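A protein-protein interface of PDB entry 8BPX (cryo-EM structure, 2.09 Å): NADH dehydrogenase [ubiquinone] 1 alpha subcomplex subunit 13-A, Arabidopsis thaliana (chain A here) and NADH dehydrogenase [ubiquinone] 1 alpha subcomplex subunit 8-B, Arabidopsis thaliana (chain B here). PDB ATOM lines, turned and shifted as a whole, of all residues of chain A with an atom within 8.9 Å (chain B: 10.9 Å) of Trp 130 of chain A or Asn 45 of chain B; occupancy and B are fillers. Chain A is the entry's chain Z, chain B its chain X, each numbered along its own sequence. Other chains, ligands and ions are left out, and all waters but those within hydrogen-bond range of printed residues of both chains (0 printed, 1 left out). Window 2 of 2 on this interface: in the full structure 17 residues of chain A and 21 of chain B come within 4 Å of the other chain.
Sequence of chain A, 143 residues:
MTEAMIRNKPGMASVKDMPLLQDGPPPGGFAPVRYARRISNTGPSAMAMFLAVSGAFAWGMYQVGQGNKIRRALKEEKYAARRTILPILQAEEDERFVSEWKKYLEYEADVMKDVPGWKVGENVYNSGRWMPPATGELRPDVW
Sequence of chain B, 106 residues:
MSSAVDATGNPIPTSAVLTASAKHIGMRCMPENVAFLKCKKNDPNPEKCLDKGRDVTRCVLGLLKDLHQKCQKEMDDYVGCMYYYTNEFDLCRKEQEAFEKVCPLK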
ATOM      1  N   GLN A  90     -14.278 -16.135   4.295  1.00  0.00           N
ATOM      2  CA  GLN A  90     -13.855 -15.328   5.434  1.00  0.00           C
ATOM      3  C   GLN A  90     -14.936 -15.274   6.509  1.00  0.00           C
ATOM      4  O   GLN A  90     -14.626 -15.312   7.699  1.00  0.00           O
ATOM      5  CB  GLN A  90     -13.487 -13.917   4.979  1.00  0.00           C
ATOM      6  CG  GLN A  90     -12.508 -13.205   5.897  1.00  0.00           C
ATOM      7  CD  GLN A  90     -11.422 -14.119   6.429  1.00  0.00           C
ATOM      8  OE1 GLN A  90     -10.547 -14.555   5.686  1.00  0.00           O
ATOM      9  NE2 GLN A  90     -11.468 -14.408   7.723  1.00  0.00           N
ATOM     10  N   GLU A  93     -14.889 -18.482   8.400  1.00  0.00           N
ATOM     11  CA  GLU A  93     -13.739 -18.509   9.296  1.00  0.00           C
ATOM     12  C   GLU A  93     -13.957 -17.603  10.502  1.00  0.00           C
ATOM     13  O   GLU A  93     -13.553 -17.939  11.620  1.00  0.00           O
ATOM     14  CB  GLU A  93     -12.467 -18.111   8.542  1.00  0.00           C
ATOM     15  CG  GLU A  93     -11.263 -17.848   9.440  1.00  0.00           C
ATOM     16  CD  GLU A  93     -10.717 -19.097  10.122  1.00  0.00           C
ATOM     17  OE1 GLU A  93     -11.276 -20.198   9.933  1.00  0.00           O
ATOM     18  OE2 GLU A  93      -9.728 -18.971  10.869  1.00  0.00           O
ATOM     19  N   ASP A  94     -14.590 -16.448  10.293  1.00  0.00           N
ATOM     20  CA  ASP A  94     -14.851 -15.529  11.396  1.00  0.00           C
ATOM     21  C   ASP A  94     -15.794 -16.153  12.415  1.00  0.00           C
ATOM     22  O   ASP A  94     -15.557 -16.075  13.625  1.00  0.00           O
ATOM     23  CB  ASP A  94     -15.427 -14.218  10.861  1.00  0.00           C
ATOM     24  CG  ASP A  94     -14.367 -13.312  10.266  1.00  0.00           C
ATOM     25  OD1 ASP A  94     -13.171 -13.663  10.339  1.00  0.00           O
ATOM     26  OD2 ASP A  94     -14.732 -12.242   9.738  1.00  0.00           O
ATOM     27  N   PHE A  97     -13.855 -18.849  14.343  1.00  0.00           N
ATOM     28  CA  PHE A  97     -12.918 -18.295  15.309  1.00  0.00           C
ATOM     29  C   PHE A  97     -13.641 -17.675  16.495  1.00  0.00           C
ATOM     30  O   PHE A  97     -13.162 -17.767  17.627  1.00  0.00           O
ATOM     31  CB  PHE A  97     -12.009 -17.256  14.659  1.00  0.00           C
ATOM     32  CG  PHE A  97     -11.049 -16.627  15.624  1.00  0.00           C
ATOM     33  CD1 PHE A  97      -9.852 -17.251  15.931  1.00  0.00           C
ATOM     34  CD2 PHE A  97     -11.357 -15.436  16.255  1.00  0.00           C
ATOM     35  CE1 PHE A  97      -8.971 -16.685  16.830  1.00  0.00           C
ATOM     36  CE2 PHE A  97     -10.484 -14.870  17.160  1.00  0.00           C
ATOM     37  CZ  PHE A  97      -9.288 -15.493  17.443  1.00  0.00           C
ATOM     38  N   VAL A  98     -14.771 -17.009  16.256  1.00  0.00           N
ATOM     39  CA  VAL A  98     -15.491 -16.385  17.361  1.00  0.00           C
ATOM     40  C   VAL A  98     -16.013 -17.444  18.323  1.00  0.00           C
ATOM     41  O   VAL A  98     -15.895 -17.301  19.547  1.00  0.00           O
ATOM     42  CB  VAL A  98     -16.620 -15.483  16.828  1.00  0.00           C
ATOM     43  CG1 VAL A  98     -17.565 -15.100  17.949  1.00  0.00           C
ATOM     44  CG2 VAL A  98     -16.037 -14.240  16.194  1.00  0.00           C
ATOM     45  N   TRP A 101     -13.098 -18.796  20.266  1.00  0.00           N
ATOM     46  CA  TRP A 101     -12.617 -17.815  21.229  1.00  0.00           C
ATOM     47  C   TRP A 101     -13.535 -17.732  22.441  1.00  0.00           C
ATOM     48  O   TRP A 101     -13.060 -17.572  23.569  1.00  0.00           O
ATOM     49  CB  TRP A 101     -12.484 -16.445  20.565  1.00  0.00           C
ATOM     50  CG  TRP A 101     -11.821 -15.449  21.450  1.00  0.00           C
ATOM     51  CD1 TRP A 101     -12.385 -14.340  22.007  1.00  0.00           C
ATOM     52  CD2 TRP A 101     -10.464 -15.478  21.898  1.00  0.00           C
ATOM     53  NE1 TRP A 101     -11.461 -13.672  22.770  1.00  0.00           N
ATOM     54  CE2 TRP A 101     -10.272 -14.351  22.719  1.00  0.00           C
ATOM     55  CE3 TRP A 101      -9.390 -16.348  21.682  1.00  0.00           C
ATOM     56  CZ2 TRP A 101      -9.054 -14.071  23.323  1.00  0.00           C
ATOM     57  CZ3 TRP A 101      -8.179 -16.065  22.282  1.00  0.00           C
ATOM     58  CH2 TRP A 101      -8.022 -14.936  23.095  1.00  0.00           C
ATOM     59  N   GLY A 121      -9.473 -12.631  29.212  1.00  0.00           N
ATOM     60  CA  GLY A 121      -9.319 -12.115  27.860  1.00  0.00           C
ATOM     61  C   GLY A 121      -8.855 -10.676  27.800  1.00  0.00           C
ATOM     62  O   GLY A 121      -9.353  -9.901  26.975  1.00  0.00           O
ATOM     63  N   ASN A 123      -6.774  -7.602  26.713  1.00  0.00           N
ATOM     64  CA  ASN A 123      -5.955  -7.232  25.565  1.00  0.00           C
ATOM     65  C   ASN A 123      -4.612  -6.693  26.048  1.00  0.00           C
ATOM     66  O   ASN A 123      -4.564  -5.729  26.817  1.00  0.00           O
ATOM     67  CB  ASN A 123      -6.678  -6.190  24.716  1.00  0.00           C
ATOM     68  CG  ASN A 123      -6.079  -6.037  23.329  1.00  0.00           C
ATOM     69  OD1 ASN A 123      -4.925  -6.391  23.089  1.00  0.00           O
ATOM     70  ND2 ASN A 123      -6.865  -5.499  22.408  1.00  0.00           N
ATOM     71  N   TYR A 125      -2.385  -5.263  24.181  1.00  0.00           N
ATOM     72  CA  TYR A 125      -2.046  -4.047  23.454  1.00  0.00           C
ATOM     73  C   TYR A 125      -2.779  -2.856  24.056  1.00  0.00           C
ATOM     74  O   TYR A 125      -3.992  -2.911  24.280  1.00  0.00           O
ATOM     75  CB  TYR A 125      -2.393  -4.200  21.973  1.00  0.00           C
ATOM     76  CG  TYR A 125      -1.509  -5.198  21.261  1.00  0.00           C
ATOM     77  CD1 TYR A 125      -0.194  -4.883  20.947  1.00  0.00           C
ATOM     78  CD2 TYR A 125      -1.981  -6.460  20.923  1.00  0.00           C
ATOM     79  CE1 TYR A 125       0.624  -5.788  20.310  1.00  0.00           C
ATOM     80  CE2 TYR A 125      -1.169  -7.375  20.280  1.00  0.00           C
ATOM     81  CZ  TYR A 125       0.136  -7.031  19.977  1.00  0.00           C
ATOM     82  OH  TYR A 125       0.954  -7.929  19.342  1.00  0.00           O
ATOM     83  N   SER A 127      -3.336   0.081  22.660  1.00  0.00           N
ATOM     84  CA  SER A 127      -4.259   0.651  21.690  1.00  0.00           C
ATOM     85  C   SER A 127      -5.586  -0.094  21.647  1.00  0.00           C
ATOM     86  O   SER A 127      -6.581   0.463  21.176  1.00  0.00           O
ATOM     87  CB  SER A 127      -3.622   0.653  20.300  1.00  0.00           C
ATOM     88  OG  SER A 127      -3.899  -0.553  19.612  1.00  0.00           O
ATOM     89  N   GLY A 128      -5.621  -1.336  22.127  1.00  0.00           N
ATOM     90  CA  GLY A 128      -6.829  -2.128  22.114  1.00  0.00           C
ATOM     91  C   GLY A 128      -7.235  -2.646  20.755  1.00  0.00           C
ATOM     92  O   GLY A 128      -8.258  -3.331  20.655  1.00  0.00           O
ATOM     93  N   ARG A 129      -6.474  -2.348  19.709  1.00  0.00           N
ATOM     94  CA  ARG A 129      -6.810  -2.856  18.389  1.00  0.00           C
ATOM     95  C   ARG A 129      -6.618  -4.367  18.347  1.00  0.00           C
ATOM     96  O   ARG A 129      -5.743  -4.928  19.012  1.00  0.00           O
ATOM     97  CB  ARG A 129      -5.978  -2.146  17.320  1.00  0.00           C
ATOM     98  CG  ARG A 129      -5.401  -3.026  16.235  1.00  0.00           C
ATOM     99  CD  ARG A 129      -4.674  -2.175  15.205  1.00  0.00           C
ATOM    100  NE  ARG A 129      -3.397  -1.648  15.667  1.00  0.00           N
ATOM    101  CZ  ARG A 129      -2.697  -0.725  15.017  1.00  0.00           C
ATOM    102  NH1 ARG A 129      -3.131  -0.203  13.883  1.00  0.00           N
ATOM    103  NH2 ARG A 129      -1.531  -0.325  15.512  1.00  0.00           N
ATOM    104  N   TRP A 130      -7.475  -5.030  17.581  1.00  0.00           N
ATOM    105  CA  TRP A 130      -7.545  -6.481  17.604  1.00  0.00           C
ATOM    106  C   TRP A 130      -6.394  -7.090  16.815  1.00  0.00           C
ATOM    107  O   TRP A 130      -6.108  -6.672  15.691  1.00  0.00           O
ATOM    108  CB  TRP A 130      -8.880  -6.956  17.039  1.00  0.00           C
ATOM    109  CG  TRP A 130      -9.071  -8.421  17.188  1.00  0.00           C
ATOM    110  CD1 TRP A 130      -9.553  -9.076  18.281  1.00  0.00           C
ATOM    111  CD2 TRP A 130      -8.767  -9.426  16.218  1.00  0.00           C
ATOM    112  NE1 TRP A 130      -9.573 -10.427  18.050  1.00  0.00           N
ATOM    113  CE2 TRP A 130      -9.099 -10.668  16.788  1.00  0.00           C
ATOM    114  CE3 TRP A 130      -8.254  -9.394  14.917  1.00  0.00           C
ATOM    115  CZ2 TRP A 130      -8.932 -11.870  16.105  1.00  0.00           C
ATOM    116  CZ3 TRP A 130      -8.090 -10.586  14.241  1.00  0.00           C
ATOM    117  CH2 TRP A 130      -8.426 -11.807  14.836  1.00  0.00           C
ATOM    118  N   MET A 131      -5.741  -8.082  17.410  1.00  0.00           N
ATOM    119  CA  MET A 131      -4.733  -8.892  16.749  1.00  0.00           C
ATOM    120  C   MET A 131      -5.063 -10.361  16.958  1.00  0.00           C
ATOM    121  O   MET A 131      -5.582 -10.739  18.013  1.00  0.00           O
ATOM    122  CB  MET A 131      -3.326  -8.598  17.294  1.00  0.00           C
ATOM    123  CG  MET A 131      -2.867  -7.155  17.108  1.00  0.00           C
ATOM    124  SD  MET A 131      -2.395  -6.742  15.418  1.00  0.00           S
ATOM    125  CE  MET A 131      -1.110  -7.949  15.105  1.00  0.00           C
ATOM    126  N   PRO A 132      -4.785 -11.210  15.971  1.00  0.00           N
ATOM    127  CA  PRO A 132      -4.992 -12.641  16.166  1.00  0.00           C
ATOM    128  C   PRO A 132      -4.076 -13.163  17.251  1.00  0.00           C
ATOM    129  O   PRO A 132      -2.990 -12.603  17.497  1.00  0.00           O
ATOM    130  CB  PRO A 132      -4.646 -13.244  14.795  1.00  0.00           C
ATOM    131  CG  PRO A 132      -4.492 -12.114  13.852  1.00  0.00           C
ATOM    132  CD  PRO A 132      -4.260 -10.875  14.637  1.00  0.00           C
ATOM    133  N   PRO A 133      -4.474 -14.228  17.944  1.00  0.00           N
ATOM    134  CA  PRO A 133      -3.608 -14.779  18.994  1.00  0.00           C
ATOM    135  C   PRO A 133      -2.294 -15.282  18.411  1.00  0.00           C
ATOM    136  O   PRO A 133      -2.269 -15.979  17.394  1.00  0.00           O
ATOM    137  CB  PRO A 133      -4.442 -15.922  19.589  1.00  0.00           C
ATOM    138  CG  PRO A 133      -5.823 -15.762  19.031  1.00  0.00           C
ATOM    139  CD  PRO A 133      -5.679 -15.044  17.732  1.00  0.00           C
ATOM    140  N   ALA A 134      -1.197 -14.910  19.061  1.00  0.00           N
ATOM    141  CA  ALA A 134       0.116 -15.364  18.632  1.00  0.00           C
ATOM    142  C   ALA A 134       0.269 -16.854  18.916  1.00  0.00           C
ATOM    143  O   ALA A 134      -0.265 -17.381  19.894  1.00  0.00           O
ATOM    144  CB  ALA A 134       1.212 -14.564  19.335  1.00  0.00           C
ATOM    145  N   PHE B  36     -19.082  -6.443   2.861  1.00  0.00           N
ATOM    146  CA  PHE B  36     -18.260  -7.244   3.759  1.00  0.00           C
ATOM    147  C   PHE B  36     -16.799  -6.824   3.679  1.00  0.00           C
ATOM    148  O   PHE B  36     -16.120  -6.694   4.705  1.00  0.00           O
ATOM    149  CB  PHE B  36     -18.411  -8.726   3.413  1.00  0.00           C
ATOM    150  CG  PHE B  36     -17.592  -9.641   4.275  1.00  0.00           C
ATOM    151  CD1 PHE B  36     -18.032 -10.014   5.533  1.00  0.00           C
ATOM    152  CD2 PHE B  36     -16.372 -10.128   3.825  1.00  0.00           C
ATOM    153  CE1 PHE B  36     -17.277 -10.860   6.322  1.00  0.00           C
ATOM    154  CE2 PHE B  36     -15.613 -10.969   4.614  1.00  0.00           C
ATOM    155  CZ  PHE B  36     -16.067 -11.335   5.864  1.00  0.00           C
ATOM    156  N   LEU B  37     -16.295  -6.615   2.461  1.00  0.00           N
ATOM    157  CA  LEU B  37     -14.891  -6.250   2.305  1.00  0.00           C
ATOM    158  C   LEU B  37     -14.602  -4.866   2.874  1.00  0.00           C
ATOM    159  O   LEU B  37     -13.551  -4.654   3.484  1.00  0.00           O
ATOM    160  CB  LEU B  37     -14.481  -6.336   0.837  1.00  0.00           C
ATOM    161  CG  LEU B  37     -14.554  -7.749   0.259  1.00  0.00           C
ATOM    162  CD1 LEU B  37     -14.207  -7.756  -1.216  1.00  0.00           C
ATOM    163  CD2 LEU B  37     -13.640  -8.676   1.042  1.00  0.00           C
ATOM    164  N   LYS B  38     -15.518  -3.911   2.693  1.00  0.00           N
ATOM    165  CA  LYS B  38     -15.341  -2.603   3.320  1.00  0.00           C
ATOM    166  C   LYS B  38     -15.266  -2.733   4.835  1.00  0.00           C
ATOM    167  O   LYS B  38     -14.373  -2.162   5.477  1.00  0.00           O
ATOM    168  CB  LYS B  38     -16.476  -1.654   2.925  1.00  0.00           C
ATOM    169  CG  LYS B  38     -16.637  -1.422   1.441  1.00  0.00           C
ATOM    170  CD  LYS B  38     -17.093  -0.002   1.151  1.00  0.00           C
ATOM    171  CE  LYS B  38     -18.071   0.036  -0.009  1.00  0.00           C
ATOM    172  NZ  LYS B  38     -17.454   0.601  -1.239  1.00  0.00           N
ATOM    173  N   CYS B  39     -16.185  -3.502   5.426  1.00  0.00           N
ATOM    174  CA  CYS B  39     -16.192  -3.611   6.882  1.00  0.00           C
ATOM    175  C   CYS B  39     -14.930  -4.307   7.384  1.00  0.00           C
ATOM    176  O   CYS B  39     -14.368  -3.918   8.413  1.00  0.00           O
ATOM    177  CB  CYS B  39     -17.447  -4.340   7.357  1.00  0.00           C
ATOM    178  SG  CYS B  39     -17.316  -4.999   9.024  1.00  0.00           S
ATOM    179  N   LYS B  40     -14.463  -5.330   6.659  1.00  0.00           N
ATOM    180  CA  LYS B  40     -13.202  -5.979   7.007  1.00  0.00           C
ATOM    181  C   LYS B  40     -12.033  -5.009   6.892  1.00  0.00           C
ATOM    182  O   LYS B  40     -11.115  -5.034   7.720  1.00  0.00           O
ATOM    183  CB  LYS B  40     -12.973  -7.201   6.114  1.00  0.00           C
ATOM    184  CG  LYS B  40     -13.787  -8.427   6.496  1.00  0.00           C
ATOM    185  CD  LYS B  40     -13.686  -8.714   7.986  1.00  0.00           C
ATOM    186  CE  LYS B  40     -12.365  -9.370   8.343  1.00  0.00           C
ATOM    187  NZ  LYS B  40     -12.536 -10.448   9.353  1.00  0.00           N
ATOM    188  N   LYS B  41     -12.048  -4.151   5.868  1.00  0.00           N
ATOM    189  CA  LYS B  41     -11.019  -3.126   5.732  1.00  0.00           C
ATOM    190  C   LYS B  41     -10.989  -2.206   6.942  1.00  0.00           C
ATOM    191  O   LYS B  41      -9.913  -1.865   7.445  1.00  0.00           O
ATOM    192  CB  LYS B  41     -11.251  -2.312   4.460  1.00  0.00           C
ATOM    193  CG  LYS B  41     -10.008  -1.642   3.916  1.00  0.00           C
ATOM    194  CD  LYS B  41     -10.153  -1.310   2.447  1.00  0.00           C
ATOM    195  CE  LYS B  41      -9.267  -0.137   2.057  1.00  0.00           C
ATOM    196  NZ  LYS B  41      -8.006  -0.108   2.843  1.00  0.00           N
ATOM    197  N   ASN B  42     -12.160  -1.782   7.419  1.00  0.00           N
ATOM    198  CA  ASN B  42     -12.187  -0.890   8.575  1.00  0.00           C
ATOM    199  C   ASN B  42     -11.814  -1.630   9.856  1.00  0.00           C
ATOM    200  O   ASN B  42     -11.105  -1.086  10.710  1.00  0.00           O
ATOM    201  CB  ASN B  42     -13.562  -0.223   8.691  1.00  0.00           C
ATOM    202  CG  ASN B  42     -13.628   0.833   9.784  1.00  0.00           C
ATOM    203  OD1 ASN B  42     -12.814   0.857  10.707  1.00  0.00           O
ATOM    204  ND2 ASN B  42     -14.613   1.718   9.680  1.00  0.00           N
ATOM    205  N   ASP B  43     -12.275  -2.867  10.009  1.00  0.00           N
ATOM    206  CA  ASP B  43     -12.042  -3.586  11.255  1.00  0.00           C
ATOM    207  C   ASP B  43     -11.759  -5.063  11.008  1.00  0.00           C
ATOM    208  O   ASP B  43     -12.643  -5.801  10.555  1.00  0.00           O
ATOM    209  CB  ASP B  43     -13.242  -3.431  12.187  1.00  0.00           C
ATOM    210  CG  ASP B  43     -12.836  -3.137  13.614  1.00  0.00           C
ATOM    211  OD1 ASP B  43     -11.788  -3.653  14.046  1.00  0.00           O
ATOM    212  OD2 ASP B  43     -13.565  -2.392  14.300  1.00  0.00           O
ATOM    213  N   PRO B  44     -10.543  -5.533  11.298  1.00  0.00           N
ATOM    214  CA  PRO B  44     -10.237  -6.960  11.131  1.00  0.00           C
ATOM    215  C   PRO B  44     -10.792  -7.852  12.230  1.00  0.00           C
ATOM    216  O   PRO B  44     -10.704  -9.080  12.100  1.00  0.00           O
ATOM    217  CB  PRO B  44      -8.704  -6.983  11.137  1.00  0.00           C
ATOM    218  CG  PRO B  44      -8.340  -5.823  11.998  1.00  0.00           C
ATOM    219  CD  PRO B  44      -9.356  -4.757  11.695  1.00  0.00           C
ATOM    220  N   ASN B  45     -11.345  -7.291  13.298  1.00  0.00           N
ATOM    221  CA  ASN B  45     -11.884  -8.105  14.377  1.00  0.00           C
ATOM    222  C   ASN B  45     -13.072  -8.908  13.859  1.00  0.00           C
ATOM    223  O   ASN B  45     -14.056  -8.313  13.393  1.00  0.00           O
ATOM    224  CB  ASN B  45     -12.297  -7.223  15.554  1.00  0.00           C
ATOM    225  CG  ASN B  45     -12.673  -8.023  16.792  1.00  0.00           C
ATOM    226  OD1 ASN B  45     -12.566  -9.248  16.817  1.00  0.00           O
ATOM    227  ND2 ASN B  45     -13.102  -7.327  17.832  1.00  0.00           N
ATOM    228  N   PRO B  46     -13.020 -10.242  13.900  1.00  0.00           N
ATOM    229  CA  PRO B  46     -14.114 -11.040  13.321  1.00  0.00           C
ATOM    230  C   PRO B  46     -15.461 -10.810  13.980  1.00  0.00           C
ATOM    231  O   PRO B  46     -16.492 -10.939  13.309  1.00  0.00           O
ATOM    232  CB  PRO B  46     -13.632 -12.486  13.516  1.00  0.00           C
ATOM    233  CG  PRO B  46     -12.567 -12.407  14.567  1.00  0.00           C
ATOM    234  CD  PRO B  46     -11.912 -11.084  14.376  1.00  0.00           C
ATOM    235  N   GLU B  47     -15.488 -10.485  15.274  1.00  0.00           N
ATOM    236  CA  GLU B  47     -16.763 -10.326  15.968  1.00  0.00           C
ATOM    237  C   GLU B  47     -17.529  -9.128  15.418  1.00  0.00           C
ATOM    238  O   GLU B  47     -18.755  -9.185  15.267  1.00  0.00           O
ATOM    239  CB  GLU B  47     -16.505 -10.222  17.480  1.00  0.00           C
ATOM    240  CG  GLU B  47     -17.712 -10.301  18.447  1.00  0.00           C
ATOM    241  CD  GLU B  47     -18.850  -9.335  18.169  1.00  0.00           C
ATOM    242  OE1 GLU B  47     -20.022  -9.733  18.341  1.00  0.00           O
ATOM    243  OE2 GLU B  47     -18.579  -8.156  17.859  1.00  0.00           O
ATOM    244  N   LYS B  48     -16.822  -8.058  15.066  1.00  0.00           N
ATOM    245  CA  LYS B  48     -17.429  -6.820  14.600  1.00  0.00           C
ATOM    246  C   LYS B  48     -17.819  -6.854  13.119  1.00  0.00           C
ATOM    247  O   LYS B  48     -17.987  -5.789  12.519  1.00  0.00           O
ATOM    248  CB  LYS B  48     -16.480  -5.648  14.858  1.00  0.00           C
ATOM    249  CG  LYS B  48     -16.135  -5.452  16.321  1.00  0.00           C
ATOM    250  CD  LYS B  48     -15.965  -3.982  16.655  1.00  0.00           C
ATOM    251  CE  LYS B  48     -15.695  -3.775  18.135  1.00  0.00           C
ATOM    252  NZ  LYS B  48     -16.212  -4.896  18.966  1.00  0.00           N
ATOM    253  N   CYS B  49     -17.953  -8.040  12.522  1.00  0.00           N
ATOM    254  CA  CYS B  49     -18.285  -8.157  11.106  1.00  0.00           C
ATOM    255  C   CYS B  49     -19.279  -9.284  10.836  1.00  0.00           C
ATOM    256  O   CYS B  49     -19.559  -9.577   9.667  1.00  0.00           O
ATOM    257  CB  CYS B  49     -16.998  -8.364  10.291  1.00  0.00           C
ATOM    258  SG  CYS B  49     -17.148  -8.283   8.493  1.00  0.00           S
ATOM    259  N   LEU B  50     -19.837  -9.905  11.878  1.00  0.00           N
ATOM    260  CA  LEU B  50     -20.642 -11.109  11.696  1.00  0.00           C
ATOM    261  C   LEU B  50     -21.905 -10.847  10.883  1.00  0.00           C
ATOM    262  O   LEU B  50     -22.353 -11.728  10.141  1.00  0.00           O
ATOM    263  CB  LEU B  50     -20.998 -11.704  13.061  1.00  0.00           C
ATOM    264  CG  LEU B  50     -19.820 -12.356  13.791  1.00  0.00           C
ATOM    265  CD1 LEU B  50     -20.242 -12.925  15.132  1.00  0.00           C
ATOM    266  CD2 LEU B  50     -19.178 -13.434  12.925  1.00  0.00           C
ATOM    267  N   ASP B  51     -22.490  -9.654  11.003  1.00  0.00           N
ATOM    268  CA  ASP B  51     -23.739  -9.362  10.300  1.00  0.00           C
ATOM    269  C   ASP B  51     -23.542  -9.330   8.786  1.00  0.00           C
ATOM    270  O   ASP B  51     -24.298  -9.964   8.037  1.00  0.00           O
ATOM    271  CB  ASP B  51     -24.311  -8.034  10.794  1.00  0.00           C
ATOM    272  CG  ASP B  51     -23.284  -6.919  10.787  1.00  0.00           C
ATOM    273  OD1 ASP B  51     -22.072  -7.227  10.819  1.00  0.00           O
ATOM    274  OD2 ASP B  51     -23.685  -5.737  10.754  1.00  0.00           O
ATOM    275  N   LYS B  52     -22.543  -8.578   8.319  1.00  0.00           N
ATOM    276  CA  LYS B  52     -22.235  -8.568   6.894  1.00  0.00           C
ATOM    277  C   LYS B  52     -21.875  -9.962   6.403  1.00  0.00           C
ATOM    278  O   LYS B  52     -22.217 -10.333   5.272  1.00  0.00           O
ATOM    279  CB  LYS B  52     -21.097  -7.586   6.609  1.00  0.00           C
ATOM    280  CG  LYS B  52     -21.564  -6.216   6.161  1.00  0.00           C
ATOM    281  CD  LYS B  52     -21.804  -5.306   7.347  1.00  0.00           C
ATOM    282  CE  LYS B  52     -22.376  -3.967   6.914  1.00  0.00           C
ATOM    283  NZ  LYS B  52     -21.411  -3.193   6.087  1.00  0.00           N
ATOM    284  N   GLY B  53     -21.206 -10.750   7.246  1.00  0.00           N
ATOM    285  CA  GLY B  53     -20.922 -12.128   6.887  1.00  0.00           C
ATOM    286  C   GLY B  53     -22.180 -12.953   6.698  1.00  0.00           C
ATOM    287  O   GLY B  53     -22.266 -13.765   5.775  1.00  0.00           O
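Of the 17 printed residues of chain A, 5 touch a printed residue of chain B.
Printed residues of chain B that touch a printed residue of chain A: Phe 36, Lys 40, Pro 44, Asn 45, Pro 46 and Glu 47.
Hydrophobic or aromatic side chains of chain B that line the printed part of chain A: Phe 36 and Pro 46.
Among the printed residues, 8 pairs touch across the chains.
Of chain B, only Pro 44, Asn 45 and Pro 46 come within 4 Å of Trp 130 of chain A.
Of chain A, only Trp 130 (3.4 Å) comes within 4 Å of Asn 45 of chain B.
Gly 128 of chain A touches none of the printed residues of chain B.
No residue of chain B comes within 4 Å of Met 131 of chain A.
No residue of chain B comes within 4 Å of Pro 132 of chain A.
Pro 44 of chain B touches one residue of chain A.
No residue of chain A comes within 4 Å of Lys 48 of chain B.
Of the printed residues of chain A, Pro 46 of chain B touches Asp 94, Phe 97 and Trp 130.
Of the printed residues of chain B, Asp 94 of chain A touches Lys 40 and Pro 46.
Glu 93 of chain A touches none of the printed residues of chain B.
The nearest residue of chain B that does not touch Trp 130 of chain A is Asp 43 of chain B (5.3 Å).
The nearest residue of chain A that does not touch Asn 45 of chain B is Asp 94 of chain A (5.4 Å).
The nearest printed residue of chain A that does not touch Glu 47 of chain B is Asp 94 of chain A (5.8 Å).
NE2 of Gln 90 of chain A lies within hydrogen-bond range of OD1 of Asp 94 of chain A, at 3.2 Å.
Gln 90 of chain A touches Phe 36 of chain B (CB to CE2, 3.7 Å).
Asp 94 of chain A touches Pro 46 of chain B (OD1 to CB, 3.4 Å).
Phe 97 of chain A touches Pro 46 of chain B.
Val 98 of chain A touches Glu 47 of chain B.
O of Pro 44 of chain B touches CZ3 of Trp 130 of chain A (3.7 Å).
CZ2 of Trp 130 of chain A touches CD of Pro 46 of chain B, at 3.5 Å.
NZ of Lys 40 of chain B lies within salt-bridge range of OD2 of Asp 94 of chain A.
NE1 of Trp 130 of chain A sits close to OD1 of Asn 45 of chain B (3.4 Å).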
